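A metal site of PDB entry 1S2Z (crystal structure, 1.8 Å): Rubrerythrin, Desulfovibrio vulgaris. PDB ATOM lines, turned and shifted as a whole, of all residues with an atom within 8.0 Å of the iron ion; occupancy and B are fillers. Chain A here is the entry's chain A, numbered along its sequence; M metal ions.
OD1 of Asn 160 lies close to SG of Cys 177 (3.3 Å).
A ring nitrogen (ND1) of His 179 is in hydrogen-bond range of the backbone carbonyl oxygen of Cys 177, 3.0 Å away.
N of Cys 174 is in hydrogen-bond range of O of His 179, 2.8 Å away.
The side-chain sulfur of Cys 158 lies close to the backbone NH of Asn 160, at 3.5 Å.
SG of Cys 161 lies close to N of Tyr 163 (3.5 Å).
The side-chain sulfur of Cys 174 lies close to the backbone NH of Ala 176, 3.5 Å away.
N of Cys 158 lies within hydrogen-bond range of O of Tyr 163, 2.8 Å away.
The iron ion is bound by the side-chain sulfur (SG) of Cys 161, the side-chain sulfur (SG) of Cys 174, the side-chain sulfur (SG) of Cys 177 and the side-chain sulfur (SG) of Cys 158.
The iron ion has four donor atoms within binding distance.
The nearest printed residue that does not touch the iron ion is Tyr 163 (4.3 Å).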
ATOM      1  N   ARG A 157       3.013  23.302 -17.655  1.00  0.00           N
ATOM      2  CA  ARG A 157       2.947  23.782 -16.275  1.00  0.00           C
ATOM      3  C   ARG A 157       1.630  23.440 -15.615  1.00  0.00           C
ATOM      4  O   ARG A 157       0.569  23.564 -16.213  1.00  0.00           O
ATOM      5  CB  ARG A 157       3.156  25.302 -16.223  1.00  0.00           C
ATOM      6  CG  ARG A 157       3.309  25.837 -14.794  1.00  0.00           C
ATOM      7  CD  ARG A 157       3.335  27.359 -14.741  1.00  0.00           C
ATOM      8  NE  ARG A 157       2.028  27.948 -15.027  1.00  0.00           N
ATOM      9  CZ  ARG A 157       1.398  28.813 -14.235  1.00  0.00           C
ATOM     10  NH1 ARG A 157       1.943  29.204 -13.100  1.00  0.00           N
ATOM     11  NH2 ARG A 157       0.205  29.282 -14.593  1.00  0.00           N
ATOM     12  N   CYS A 158       1.708  22.978 -14.361  1.00  0.00           N
ATOM     13  CA  CYS A 158       0.511  22.660 -13.602  1.00  0.00           C
ATOM     14  C   CYS A 158      -0.002  23.994 -13.047  1.00  0.00           C
ATOM     15  O   CYS A 158       0.703  24.662 -12.300  1.00  0.00           O
ATOM     16  CB  CYS A 158       0.842  21.723 -12.441  1.00  0.00           C
ATOM     17  SG  CYS A 158      -0.543  21.446 -11.318  1.00  0.00           S
ATOM     18  N   ARG A 159      -1.227  24.379 -13.408  1.00  0.00           N
ATOM     19  CA  ARG A 159      -1.771  25.646 -12.912  1.00  0.00           C
ATOM     20  C   ARG A 159      -2.056  25.620 -11.418  1.00  0.00           C
ATOM     21  O   ARG A 159      -2.055  26.658 -10.754  1.00  0.00           O
ATOM     22  CB  ARG A 159      -3.061  25.999 -13.683  1.00  0.00           C
ATOM     23  CG  ARG A 159      -2.826  26.443 -15.116  1.00  0.00           C
ATOM     24  CD  ARG A 159      -4.142  26.833 -15.794  1.00  0.00           C
ATOM     25  NE  ARG A 159      -4.773  27.993 -15.160  1.00  0.00           N
ATOM     26  CZ  ARG A 159      -4.322  29.235 -15.235  1.00  0.00           C
ATOM     27  NH1 ARG A 159      -3.210  29.516 -15.918  1.00  0.00           N
ATOM     28  NH2 ARG A 159      -4.963  30.210 -14.613  1.00  0.00           N
ATOM     29  N   ASN A 160      -2.271  24.422 -10.866  1.00  0.00           N
ATOM     30  CA  ASN A 160      -2.573  24.285  -9.451  1.00  0.00           C
ATOM     31  C   ASN A 160      -1.364  24.525  -8.521  1.00  0.00           C
ATOM     32  O   ASN A 160      -1.515  25.193  -7.490  1.00  0.00           O
ATOM     33  CB  ASN A 160      -3.153  22.898  -9.177  1.00  0.00           C
ATOM     34  CG  ASN A 160      -3.647  22.733  -7.751  1.00  0.00           C
ATOM     35  OD1 ASN A 160      -3.105  21.941  -6.971  1.00  0.00           O
ATOM     36  ND2 ASN A 160      -4.685  23.484  -7.402  1.00  0.00           N
ATOM     37  N   CYS A 161      -0.199  24.011  -8.884  1.00  0.00           N
ATOM     38  CA  CYS A 161       0.983  24.154  -8.031  1.00  0.00           C
ATOM     39  C   CYS A 161       2.249  24.680  -8.691  1.00  0.00           C
ATOM     40  O   CYS A 161       3.246  24.942  -8.000  1.00  0.00           O
ATOM     41  CB  CYS A 161       1.308  22.802  -7.379  1.00  0.00           C
ATOM     42  SG  CYS A 161       2.122  21.620  -8.503  1.00  0.00           S
ATOM     43  N   GLY A 162       2.243  24.824 -10.014  1.00  0.00           N
ATOM     44  CA  GLY A 162       3.419  25.348 -10.686  1.00  0.00           C
ATOM     45  C   GLY A 162       4.442  24.321 -11.146  1.00  0.00           C
ATOM     46  O   GLY A 162       5.481  24.689 -11.677  1.00  0.00           O
ATOM     47  N   TYR A 163       4.162  23.039 -10.918  1.00  0.00           N
ATOM     48  CA  TYR A 163       5.103  22.002 -11.354  1.00  0.00           C
ATOM     49  C   TYR A 163       5.291  22.102 -12.863  1.00  0.00           C
ATOM     50  O   TYR A 163       4.341  22.368 -13.595  1.00  0.00           O
ATOM     51  CB  TYR A 163       4.579  20.609 -11.004  1.00  0.00           C
ATOM     52  CG  TYR A 163       5.479  19.496 -11.492  1.00  0.00           C
ATOM     53  CD1 TYR A 163       6.711  19.246 -10.890  1.00  0.00           C
ATOM     54  CD2 TYR A 163       5.122  18.729 -12.603  1.00  0.00           C
ATOM     55  CE1 TYR A 163       7.565  18.252 -11.366  1.00  0.00           C
ATOM     56  CE2 TYR A 163       5.966  17.728 -13.087  1.00  0.00           C
ATOM     57  CZ  TYR A 163       7.184  17.500 -12.460  1.00  0.00           C
ATOM     58  OH  TYR A 163       8.017  16.512 -12.942  1.00  0.00           O
ATOM     59  N   VAL A 164       6.520  21.887 -13.328  1.00  0.00           N
ATOM     60  CA  VAL A 164       6.816  21.932 -14.749  1.00  0.00           C
ATOM     61  C   VAL A 164       7.198  20.532 -15.222  1.00  0.00           C
ATOM     62  O   VAL A 164       8.093  19.894 -14.662  1.00  0.00           O
ATOM     63  CB  VAL A 164       7.980  22.895 -15.050  1.00  0.00           C
ATOM     64  CG1 VAL A 164       8.358  22.828 -16.532  1.00  0.00           C
ATOM     65  CG2 VAL A 164       7.590  24.321 -14.680  1.00  0.00           C
ATOM     66  N   LEU A 173      -1.308  12.665 -13.876  1.00  0.00           N
ATOM     67  CA  LEU A 173      -1.355  13.218 -12.529  1.00  0.00           C
ATOM     68  C   LEU A 173      -0.119  14.077 -12.290  1.00  0.00           C
ATOM     69  O   LEU A 173       0.985  13.693 -12.696  1.00  0.00           O
ATOM     70  CB  LEU A 173      -1.395  12.102 -11.479  1.00  0.00           C
ATOM     71  CG  LEU A 173      -2.680  11.285 -11.367  1.00  0.00           C
ATOM     72  CD1 LEU A 173      -2.493  10.205 -10.300  1.00  0.00           C
ATOM     73  CD2 LEU A 173      -3.830  12.205 -11.004  1.00  0.00           C
ATOM     74  N   CYS A 174      -0.304  15.216 -11.641  1.00  0.00           N
ATOM     75  CA  CYS A 174       0.834  16.076 -11.341  1.00  0.00           C
ATOM     76  C   CYS A 174       1.629  15.376 -10.236  1.00  0.00           C
ATOM     77  O   CYS A 174       1.083  15.034  -9.191  1.00  0.00           O
ATOM     78  CB  CYS A 174       0.365  17.445 -10.833  1.00  0.00           C
ATOM     79  SG  CYS A 174       1.738  18.526 -10.347  1.00  0.00           S
ATOM     80  N   PRO A 175       2.927  15.150 -10.455  1.00  0.00           N
ATOM     81  CA  PRO A 175       3.708  14.473  -9.418  1.00  0.00           C
ATOM     82  C   PRO A 175       3.911  15.295  -8.129  1.00  0.00           C
ATOM     83  O   PRO A 175       4.255  14.739  -7.085  1.00  0.00           O
ATOM     84  CB  PRO A 175       5.026  14.148 -10.124  1.00  0.00           C
ATOM     85  CG  PRO A 175       5.164  15.275 -11.091  1.00  0.00           C
ATOM     86  CD  PRO A 175       3.762  15.433 -11.642  1.00  0.00           C
ATOM     87  N   ALA A 176       3.690  16.595  -8.220  1.00  0.00           N
ATOM     88  CA  ALA A 176       3.869  17.473  -7.064  1.00  0.00           C
ATOM     89  C   ALA A 176       2.598  17.640  -6.218  1.00  0.00           C
ATOM     90  O   ALA A 176       2.647  17.517  -4.994  1.00  0.00           O
ATOM     91  CB  ALA A 176       4.378  18.843  -7.517  1.00  0.00           C
ATOM     92  N   CYS A 177       1.463  17.929  -6.861  1.00  0.00           N
ATOM     93  CA  CYS A 177       0.226  18.140  -6.110  1.00  0.00           C
ATOM     94  C   CYS A 177      -0.840  17.064  -6.294  1.00  0.00           C
ATOM     95  O   CYS A 177      -1.914  17.142  -5.704  1.00  0.00           O
ATOM     96  CB  CYS A 177      -0.374  19.503  -6.456  1.00  0.00           C
ATOM     97  SG  CYS A 177      -1.099  19.601  -8.100  1.00  0.00           S
ATOM     98  N   ALA A 178      -0.541  16.061  -7.114  1.00  0.00           N
ATOM     99  CA  ALA A 178      -1.454  14.949  -7.373  1.00  0.00           C
ATOM    100  C   ALA A 178      -2.758  15.308  -8.078  1.00  0.00           C
ATOM    101  O   ALA A 178      -3.670  14.476  -8.147  1.00  0.00           O
ATOM    102  CB  ALA A 178      -1.759  14.216  -6.058  1.00  0.00           C
ATOM    103  N   HIS A 179      -2.870  16.533  -8.570  1.00  0.00           N
ATOM    104  CA  HIS A 179      -4.086  16.919  -9.282  1.00  0.00           C
ATOM    105  C   HIS A 179      -4.034  16.353 -10.702  1.00  0.00           C
ATOM    106  O   HIS A 179      -2.957  16.087 -11.226  1.00  0.00           O
ATOM    107  CB  HIS A 179      -4.243  18.441  -9.293  1.00  0.00           C
ATOM    108  CG  HIS A 179      -4.760  18.997  -8.007  1.00  0.00           C
ATOM    109  ND1 HIS A 179      -4.170  18.732  -6.788  1.00  0.00           N
ATOM    110  CD2 HIS A 179      -5.840  19.781  -7.737  1.00  0.00           C
ATOM    111  CE1 HIS A 179      -4.856  19.328  -5.825  1.00  0.00           C
ATOM    112  NE2 HIS A 179      -5.864  19.978  -6.378  1.00  0.00           N
ATOM    113  N   PRO A 180      -5.201  16.146 -11.336  1.00  0.00           N
ATOM    114  CA  PRO A 180      -5.258  15.594 -12.692  1.00  0.00           C
ATOM    115  C   PRO A 180      -4.709  16.451 -13.828  1.00  0.00           C
ATOM    116  O   PRO A 180      -4.489  17.651 -13.686  1.00  0.00           O
ATOM    117  CB  PRO A 180      -6.735  15.263 -12.874  1.00  0.00           C
ATOM    118  CG  PRO A 180      -7.402  16.327 -12.074  1.00  0.00           C
ATOM    119  CD  PRO A 180      -6.557  16.391 -10.811  1.00  0.00           C
ATOM    120  N   HIS A 183      -5.313  20.240 -15.084  1.00  0.00           N
ATOM    121  CA  HIS A 183      -4.701  21.478 -14.609  1.00  0.00           C
ATOM    122  C   HIS A 183      -3.493  21.964 -15.395  1.00  0.00           C
ATOM    123  O   HIS A 183      -3.011  23.073 -15.162  1.00  0.00           O
ATOM    124  CB  HIS A 183      -4.307  21.302 -13.134  1.00  0.00           C
ATOM    125  CG  HIS A 183      -5.482  21.146 -12.217  1.00  0.00           C
ATOM    126  ND1 HIS A 183      -6.063  22.213 -11.555  1.00  0.00           N
ATOM    127  CD2 HIS A 183      -6.235  20.069 -11.905  1.00  0.00           C
ATOM    128  CE1 HIS A 183      -7.119  21.801 -10.886  1.00  0.00           C
ATOM    129  NE2 HIS A 183      -7.247  20.497 -11.082  1.00  0.00           N
ATOM    130  N   PHE A 184      -3.021  21.158 -16.344  1.00  0.00           N
ATOM    131  CA  PHE A 184      -1.851  21.539 -17.122  1.00  0.00           C
ATOM    132  C   PHE A 184      -2.085  22.422 -18.337  1.00  0.00           C
ATOM    133  O   PHE A 184      -3.131  22.359 -18.991  1.00  0.00           O
ATOM    134  CB  PHE A 184      -1.075  20.288 -17.553  1.00  0.00           C
ATOM    135  CG  PHE A 184      -0.319  19.629 -16.434  1.00  0.00           C
ATOM    136  CD1 PHE A 184      -0.941  18.725 -15.581  1.00  0.00           C
ATOM    137  CD2 PHE A 184       1.030  19.941 -16.214  1.00  0.00           C
ATOM    138  CE1 PHE A 184      -0.237  18.133 -14.528  1.00  0.00           C
ATOM    139  CE2 PHE A 184       1.737  19.358 -15.160  1.00  0.00           C
ATOM    140  CZ  PHE A 184       1.098  18.451 -14.321  1.00  0.00           C
HETATM  141 FE    FE M   1       0.571  20.343  -9.568  1.00  0.00          FE
